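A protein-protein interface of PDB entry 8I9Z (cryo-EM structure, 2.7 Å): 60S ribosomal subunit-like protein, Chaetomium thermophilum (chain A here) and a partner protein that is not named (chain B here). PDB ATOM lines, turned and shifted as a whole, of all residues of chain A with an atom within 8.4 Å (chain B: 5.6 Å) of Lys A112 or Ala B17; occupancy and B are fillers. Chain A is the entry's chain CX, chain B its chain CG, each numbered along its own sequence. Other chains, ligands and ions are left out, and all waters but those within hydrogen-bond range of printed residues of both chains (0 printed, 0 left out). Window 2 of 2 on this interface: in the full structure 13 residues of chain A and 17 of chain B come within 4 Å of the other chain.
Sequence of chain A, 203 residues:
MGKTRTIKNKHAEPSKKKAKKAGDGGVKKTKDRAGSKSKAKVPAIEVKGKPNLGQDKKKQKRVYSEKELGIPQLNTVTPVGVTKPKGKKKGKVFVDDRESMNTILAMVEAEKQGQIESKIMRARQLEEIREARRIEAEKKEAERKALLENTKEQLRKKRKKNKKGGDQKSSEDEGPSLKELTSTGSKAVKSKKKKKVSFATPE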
ATOM      1  N   LEU A 105     -19.411  21.706  20.130  1.00  0.00           N
ATOM      2  CA  LEU A 105     -19.547  20.256  20.056  1.00  0.00           C
ATOM      3  C   LEU A 105     -18.222  19.547  20.307  1.00  0.00           C
ATOM      4  O   LEU A 105     -18.203  18.429  20.834  1.00  0.00           O
ATOM      5  CB  LEU A 105     -20.101  19.869  18.692  1.00  0.00           C
ATOM      6  CG  LEU A 105     -20.725  18.490  18.594  1.00  0.00           C
ATOM      7  CD1 LEU A 105     -21.815  18.365  19.627  1.00  0.00           C
ATOM      8  CD2 LEU A 105     -21.281  18.303  17.212  1.00  0.00           C
ATOM      9  N   ALA A 106     -17.108  20.175  19.926  1.00  0.00           N
ATOM     10  CA  ALA A 106     -15.801  19.557  20.121  1.00  0.00           C
ATOM     11  C   ALA A 106     -15.453  19.435  21.598  1.00  0.00           C
ATOM     12  O   ALA A 106     -14.863  18.435  22.020  1.00  0.00           O
ATOM     13  CB  ALA A 106     -14.730  20.355  19.381  1.00  0.00           C
ATOM     14  N   MET A 107     -15.806  20.440  22.402  1.00  0.00           N
ATOM     15  CA  MET A 107     -15.487  20.376  23.825  1.00  0.00           C
ATOM     16  C   MET A 107     -16.418  19.423  24.569  1.00  0.00           C
ATOM     17  O   MET A 107     -16.026  18.836  25.582  1.00  0.00           O
ATOM     18  CB  MET A 107     -15.527  21.765  24.464  1.00  0.00           C
ATOM     19  CG  MET A 107     -14.469  22.747  23.982  1.00  0.00           C
ATOM     20  SD  MET A 107     -14.850  24.449  24.446  1.00  0.00           S
ATOM     21  CE  MET A 107     -15.212  25.222  22.881  1.00  0.00           C
ATOM     22  N   VAL A 108     -17.660  19.273  24.101  1.00  0.00           N
ATOM     23  CA  VAL A 108     -18.590  18.342  24.742  1.00  0.00           C
ATOM     24  C   VAL A 108     -18.144  16.902  24.521  1.00  0.00           C
ATOM     25  O   VAL A 108     -18.156  16.081  25.444  1.00  0.00           O
ATOM     26  CB  VAL A 108     -20.026  18.573  24.238  1.00  0.00           C
ATOM     27  CG1 VAL A 108     -20.993  17.650  24.954  1.00  0.00           C
ATOM     28  CG2 VAL A 108     -20.443  20.001  24.481  1.00  0.00           C
ATOM     29  N   GLU A 109     -17.739  16.577  23.292  1.00  0.00           N
ATOM     30  CA  GLU A 109     -17.285  15.224  22.994  1.00  0.00           C
ATOM     31  C   GLU A 109     -15.960  14.918  23.678  1.00  0.00           C
ATOM     32  O   GLU A 109     -15.699  13.770  24.055  1.00  0.00           O
ATOM     33  CB  GLU A 109     -17.165  15.036  21.484  1.00  0.00           C
ATOM     34  CG  GLU A 109     -18.398  14.438  20.833  1.00  0.00           C
ATOM     35  CD  GLU A 109     -18.088  13.764  19.511  1.00  0.00           C
ATOM     36  OE1 GLU A 109     -16.911  13.785  19.093  1.00  0.00           O
ATOM     37  OE2 GLU A 109     -19.021  13.212  18.890  1.00  0.00           O
ATOM     38  N   ALA A 110     -15.106  15.929  23.842  1.00  0.00           N
ATOM     39  CA  ALA A 110     -13.817  15.709  24.487  1.00  0.00           C
ATOM     40  C   ALA A 110     -13.982  15.476  25.980  1.00  0.00           C
ATOM     41  O   ALA A 110     -13.273  14.658  26.576  1.00  0.00           O
ATOM     42  CB  ALA A 110     -12.893  16.897  24.232  1.00  0.00           C
ATOM     43  N   GLU A 111     -14.918  16.195  26.603  1.00  0.00           N
ATOM     44  CA  GLU A 111     -15.111  16.078  28.043  1.00  0.00           C
ATOM     45  C   GLU A 111     -15.695  14.724  28.416  1.00  0.00           C
ATOM     46  O   GLU A 111     -15.352  14.156  29.458  1.00  0.00           O
ATOM     47  CB  GLU A 111     -16.012  17.208  28.536  1.00  0.00           C
ATOM     48  CG  GLU A 111     -15.270  18.311  29.268  1.00  0.00           C
ATOM     49  CD  GLU A 111     -16.143  19.041  30.269  1.00  0.00           C
ATOM     50  OE1 GLU A 111     -17.093  18.424  30.794  1.00  0.00           O
ATOM     51  OE2 GLU A 111     -15.879  20.234  30.529  1.00  0.00           O
ATOM     52  N   LYS A 112     -16.582  14.192  27.577  1.00  0.00           N
ATOM     53  CA  LYS A 112     -17.235  12.929  27.896  1.00  0.00           C
ATOM     54  C   LYS A 112     -16.297  11.748  27.691  1.00  0.00           C
ATOM     55  O   LYS A 112     -16.418  10.729  28.378  1.00  0.00           O
ATOM     56  CB  LYS A 112     -18.492  12.766  27.047  1.00  0.00           C
ATOM     57  CG  LYS A 112     -19.751  13.285  27.711  1.00  0.00           C
ATOM     58  CD  LYS A 112     -20.942  12.400  27.398  1.00  0.00           C
ATOM     59  CE  LYS A 112     -20.692  10.971  27.841  1.00  0.00           C
ATOM     60  NZ  LYS A 112     -20.952  10.803  29.295  1.00  0.00           N
ATOM     61  N   GLN A 113     -15.366  11.862  26.743  1.00  0.00           N
ATOM     62  CA  GLN A 113     -14.482  10.746  26.428  1.00  0.00           C
ATOM     63  C   GLN A 113     -13.487  10.496  27.555  1.00  0.00           C
ATOM     64  O   GLN A 113     -13.299   9.354  27.989  1.00  0.00           O
ATOM     65  CB  GLN A 113     -13.758  11.019  25.114  1.00  0.00           C
ATOM     66  CG  GLN A 113     -12.638  10.067  24.813  1.00  0.00           C
ATOM     67  CD  GLN A 113     -12.688   9.568  23.388  1.00  0.00           C
ATOM     68  OE1 GLN A 113     -12.967  10.330  22.466  1.00  0.00           O
ATOM     69  NE2 GLN A 113     -12.421   8.282  23.200  1.00  0.00           N
ATOM     70  N   GLY A 114     -12.854  11.548  28.048  1.00  0.00           N
ATOM     71  CA  GLY A 114     -12.030  11.417  29.238  1.00  0.00           C
ATOM     72  C   GLY A 114     -10.616  11.006  28.907  1.00  0.00           C
ATOM     73  O   GLY A 114     -10.022  11.492  27.941  1.00  0.00           O
ATOM     74  N   GLN A 115     -10.070  10.104  29.715  1.00  0.00           N
ATOM     75  CA  GLN A 115      -8.655   9.764  29.634  1.00  0.00           C
ATOM     76  C   GLN A 115      -8.404   8.771  28.507  1.00  0.00           C
ATOM     77  O   GLN A 115      -9.044   7.718  28.440  1.00  0.00           O
ATOM     78  CB  GLN A 115      -8.182   9.188  30.965  1.00  0.00           C
ATOM     79  CG  GLN A 115      -7.529  10.208  31.882  1.00  0.00           C
ATOM     80  CD  GLN A 115      -8.543  11.013  32.672  1.00  0.00           C
ATOM     81  OE1 GLN A 115      -9.244  10.478  33.532  1.00  0.00           O
ATOM     82  NE2 GLN A 115      -8.627  12.306  32.382  1.00  0.00           N
ATOM     83  N   GLN A 125      -7.365  14.693  19.930  1.00  0.00           N
ATOM     84  CA  GLN A 125      -8.557  15.178  20.612  1.00  0.00           C
ATOM     85  C   GLN A 125      -8.479  16.674  20.875  1.00  0.00           C
ATOM     86  O   GLN A 125      -9.509  17.357  20.890  1.00  0.00           O
ATOM     87  CB  GLN A 125      -8.749  14.413  21.915  1.00  0.00           C
ATOM     88  CG  GLN A 125     -10.160  14.403  22.425  1.00  0.00           C
ATOM     89  CD  GLN A 125     -10.237  13.953  23.863  1.00  0.00           C
ATOM     90  OE1 GLN A 125      -9.426  14.356  24.694  1.00  0.00           O
ATOM     91  NE2 GLN A 125     -11.213  13.110  24.167  1.00  0.00           N
ATOM     92  N   VAL B  12     -27.683  21.627  26.180  1.00  0.00           N
ATOM     93  CA  VAL B  12     -28.460  20.755  25.299  1.00  0.00           C
ATOM     94  C   VAL B  12     -27.582  19.650  24.723  1.00  0.00           C
ATOM     95  O   VAL B  12     -27.956  18.472  24.721  1.00  0.00           O
ATOM     96  CB  VAL B  12     -29.135  21.584  24.191  1.00  0.00           C
ATOM     97  CG1 VAL B  12     -29.602  20.698  23.056  1.00  0.00           C
ATOM     98  CG2 VAL B  12     -30.308  22.356  24.753  1.00  0.00           C
ATOM     99  N   LEU B  13     -26.390  20.011  24.249  1.00  0.00           N
ATOM    100  CA  LEU B  13     -25.517  19.018  23.638  1.00  0.00           C
ATOM    101  C   LEU B  13     -24.871  18.110  24.676  1.00  0.00           C
ATOM    102  O   LEU B  13     -24.405  17.020  24.332  1.00  0.00           O
ATOM    103  CB  LEU B  13     -24.454  19.715  22.795  1.00  0.00           C
ATOM    104  CG  LEU B  13     -24.972  20.357  21.510  1.00  0.00           C
ATOM    105  CD1 LEU B  13     -23.883  21.158  20.839  1.00  0.00           C
ATOM    106  CD2 LEU B  13     -25.504  19.300  20.573  1.00  0.00           C
ATOM    107  N   ASP B  14     -24.811  18.543  25.936  1.00  0.00           N
ATOM    108  CA  ASP B  14     -24.327  17.667  26.999  1.00  0.00           C
ATOM    109  C   ASP B  14     -25.314  16.539  27.262  1.00  0.00           C
ATOM    110  O   ASP B  14     -24.919  15.401  27.535  1.00  0.00           O
ATOM    111  CB  ASP B  14     -24.082  18.471  28.273  1.00  0.00           C
ATOM    112  CG  ASP B  14     -22.611  18.662  28.565  1.00  0.00           C
ATOM    113  OD1 ASP B  14     -21.818  17.752  28.246  1.00  0.00           O
ATOM    114  OD2 ASP B  14     -22.246  19.724  29.113  1.00  0.00           O
ATOM    115  N   LYS B  15     -26.609  16.845  27.200  1.00  0.00           N
ATOM    116  CA  LYS B  15     -27.619  15.814  27.386  1.00  0.00           C
ATOM    117  C   LYS B  15     -27.667  14.869  26.193  1.00  0.00           C
ATOM    118  O   LYS B  15     -27.914  13.668  26.350  1.00  0.00           O
ATOM    119  CB  LYS B  15     -28.981  16.462  27.629  1.00  0.00           C
ATOM    120  CG  LYS B  15     -30.077  15.489  27.982  1.00  0.00           C
ATOM    121  CD  LYS B  15     -29.790  14.774  29.280  1.00  0.00           C
ATOM    122  CE  LYS B  15     -30.035  15.662  30.469  1.00  0.00           C
ATOM    123  NZ  LYS B  15     -29.869  14.902  31.731  1.00  0.00           N
ATOM    124  N   LEU B  16     -27.423  15.390  24.991  1.00  0.00           N
ATOM    125  CA  LEU B  16     -27.432  14.541  23.807  1.00  0.00           C
ATOM    126  C   LEU B  16     -26.188  13.661  23.747  1.00  0.00           C
ATOM    127  O   LEU B  16     -26.236  12.547  23.216  1.00  0.00           O
ATOM    128  CB  LEU B  16     -27.548  15.399  22.551  1.00  0.00           C
ATOM    129  CG  LEU B  16     -28.892  16.095  22.340  1.00  0.00           C
ATOM    130  CD1 LEU B  16     -28.924  16.811  21.011  1.00  0.00           C
ATOM    131  CD2 LEU B  16     -30.023  15.103  22.434  1.00  0.00           C
ATOM    132  N   ALA B  17     -25.065  14.145  24.282  1.00  0.00           N
ATOM    133  CA  ALA B  17     -23.837  13.356  24.262  1.00  0.00           C
ATOM    134  C   ALA B  17     -23.906  12.180  25.219  1.00  0.00           C
ATOM    135  O   ALA B  17     -23.137  11.223  25.082  1.00  0.00           O
ATOM    136  CB  ALA B  17     -22.634  14.233  24.599  1.00  0.00           C
ATOM    137  N   ASN B  18     -24.809  12.235  26.195  1.00  0.00           N
ATOM    138  CA  ASN B  18     -24.964  11.126  27.126  1.00  0.00           C
ATOM    139  C   ASN B  18     -25.633   9.937  26.448  1.00  0.00           C
ATOM    140  O   ASN B  18     -25.430   8.787  26.851  1.00  0.00           O
ATOM    141  CB  ASN B  18     -25.774  11.590  28.336  1.00  0.00           C
ATOM    142  CG  ASN B  18     -25.609  10.689  29.541  1.00  0.00           C
ATOM    143  OD1 ASN B  18     -24.917   9.674  29.492  1.00  0.00           O
ATOM    144  ND2 ASN B  18     -26.250  11.063  30.642  1.00  0.00           N
ATOM    145  N   TYR B  19     -26.423  10.193  25.406  1.00  0.00           N
ATOM    146  CA  TYR B  19     -27.259   9.175  24.790  1.00  0.00           C
ATOM    147  C   TYR B  19     -26.839   8.803  23.373  1.00  0.00           C
ATOM    148  O   TYR B  19     -27.227   7.733  22.898  1.00  0.00           O
ATOM    149  CB  TYR B  19     -28.718   9.650  24.776  1.00  0.00           C
ATOM    150  CG  TYR B  19     -29.372   9.666  26.140  1.00  0.00           C
ATOM    151  CD1 TYR B  19     -29.575  10.856  26.823  1.00  0.00           C
ATOM    152  CD2 TYR B  19     -29.792   8.493  26.741  1.00  0.00           C
ATOM    153  CE1 TYR B  19     -30.167  10.874  28.068  1.00  0.00           C
ATOM    154  CE2 TYR B  19     -30.390   8.504  27.982  1.00  0.00           C
ATOM    155  CZ  TYR B  19     -30.570   9.697  28.641  1.00  0.00           C
ATOM    156  OH  TYR B  19     -31.163   9.708  29.879  1.00  0.00           O
ATOM    157  N   MET B  20     -26.062   9.642  22.687  1.00  0.00           N
ATOM    158  CA  MET B  20     -25.779   9.451  21.270  1.00  0.00           C
ATOM    159  C   MET B  20     -24.278   9.499  21.032  1.00  0.00           C
ATOM    160  O   MET B  20     -23.499   9.880  21.910  1.00  0.00           O
ATOM    161  CB  MET B  20     -26.480  10.502  20.403  1.00  0.00           C
ATOM    162  CG  MET B  20     -27.979  10.557  20.547  1.00  0.00           C
ATOM    163  SD  MET B  20     -28.755  11.744  19.433  1.00  0.00           S
ATOM    164  CE  MET B  20     -27.673  11.652  18.016  1.00  0.00           C
ATOM    165  N   LEU B  23     -22.634  13.153  17.127  1.00  0.00           N
ATOM    166  CA  LEU B  23     -23.298  14.437  17.293  1.00  0.00           C
ATOM    167  C   LEU B  23     -22.983  15.390  16.150  1.00  0.00           C
ATOM    168  O   LEU B  23     -23.766  16.308  15.881  1.00  0.00           O
ATOM    169  CB  LEU B  23     -22.920  15.057  18.633  1.00  0.00           C
ATOM    170  CG  LEU B  23     -23.437  14.356  19.886  1.00  0.00           C
ATOM    171  CD1 LEU B  23     -23.319  15.282  21.076  1.00  0.00           C
ATOM    172  CD2 LEU B  23     -24.874  13.909  19.703  1.00  0.00           C
ATOM    173  N   ARG B  95     -25.880   4.959  21.649  1.00  0.00           N
ATOM    174  CA  ARG B  95     -24.606   4.395  22.076  1.00  0.00           C
ATOM    175  C   ARG B  95     -24.796   3.027  22.713  1.00  0.00           C
ATOM    176  O   ARG B  95     -24.233   2.032  22.248  1.00  0.00           O
ATOM    177  CB  ARG B  95     -23.910   5.337  23.055  1.00  0.00           C
ATOM    178  CG  ARG B  95     -22.426   5.084  23.194  1.00  0.00           C
ATOM    179  CD  ARG B  95     -21.855   5.822  24.381  1.00  0.00           C
ATOM    180  NE  ARG B  95     -21.240   7.084  23.996  1.00  0.00           N
ATOM    181  CZ  ARG B  95     -21.732   8.273  24.305  1.00  0.00           C
ATOM    182  NH1 ARG B  95     -22.850   8.398  24.997  1.00  0.00           N
ATOM    183  NH2 ARG B  95     -21.087   9.366  23.909  1.00  0.00           N
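Of the 12 printed residues of chain A, 3 touch a printed residue of chain B. Hydrophobic or aromatic side chains of chain A that line the printed part of chain B: Leu A105 and Val A108. Printed residues of chain B that touch a printed residue of chain A: Leu B13, Asp B14, Ala B17 and Leu B23. Hydrophobic or aromatic side chains of chain B within 4 Å of the printed part of chain A: Leu B13, Ala B17 and Leu B23. Among the printed residues, no Asp or Glu carboxylate lies within 4 Å of a Lys or Arg side-chain nitrogen of the other chain.
Among the printed residues, pairs that only touch across the chains: Leu A105 with Leu B13 (3.7 Å), Leu A105 with Leu B23 (3.5 Å), Val A108 with Leu B13 (3.5 Å), Val A108 with Asp B14 (3.4 Å), Val A108 with Ala B17 (3.8 Å) and Lys A112 with Ala B17 (3.4 Å).
The backbone carbonyl oxygen of Ala B17 lies within hydrogen-bond range of the guanidinium group of Arg B95 (2.8 Å).
Of the printed residues of chain B, Leu A105 touches Leu B13 (3.7 Å) and Leu B23 (3.5 Å). Glu A109 touches none of the printed residues of chain B. Lys A112 touches just one residue of chain B: Ala B17. Val B12 touches none of the printed residues of chain A. Of the printed residues of chain A, Leu B13 touches Leu A105 and Val A108. Printed residues of chain A within 4 Å of Asp B14: Val A108 (3.4 Å). Ala B17 touches just these residues of chain A: Val A108 (3.8 Å) and Lys A112 (3.4 Å). Of the printed residues of chain A, Leu B23 touches Leu A105. The nearest residue of chain B that does not touch Lys A112 is Asn B18 (4.1 Å). The nearest residue of chain A that does not touch Ala B17 is Glu A109 (5.6 Å).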
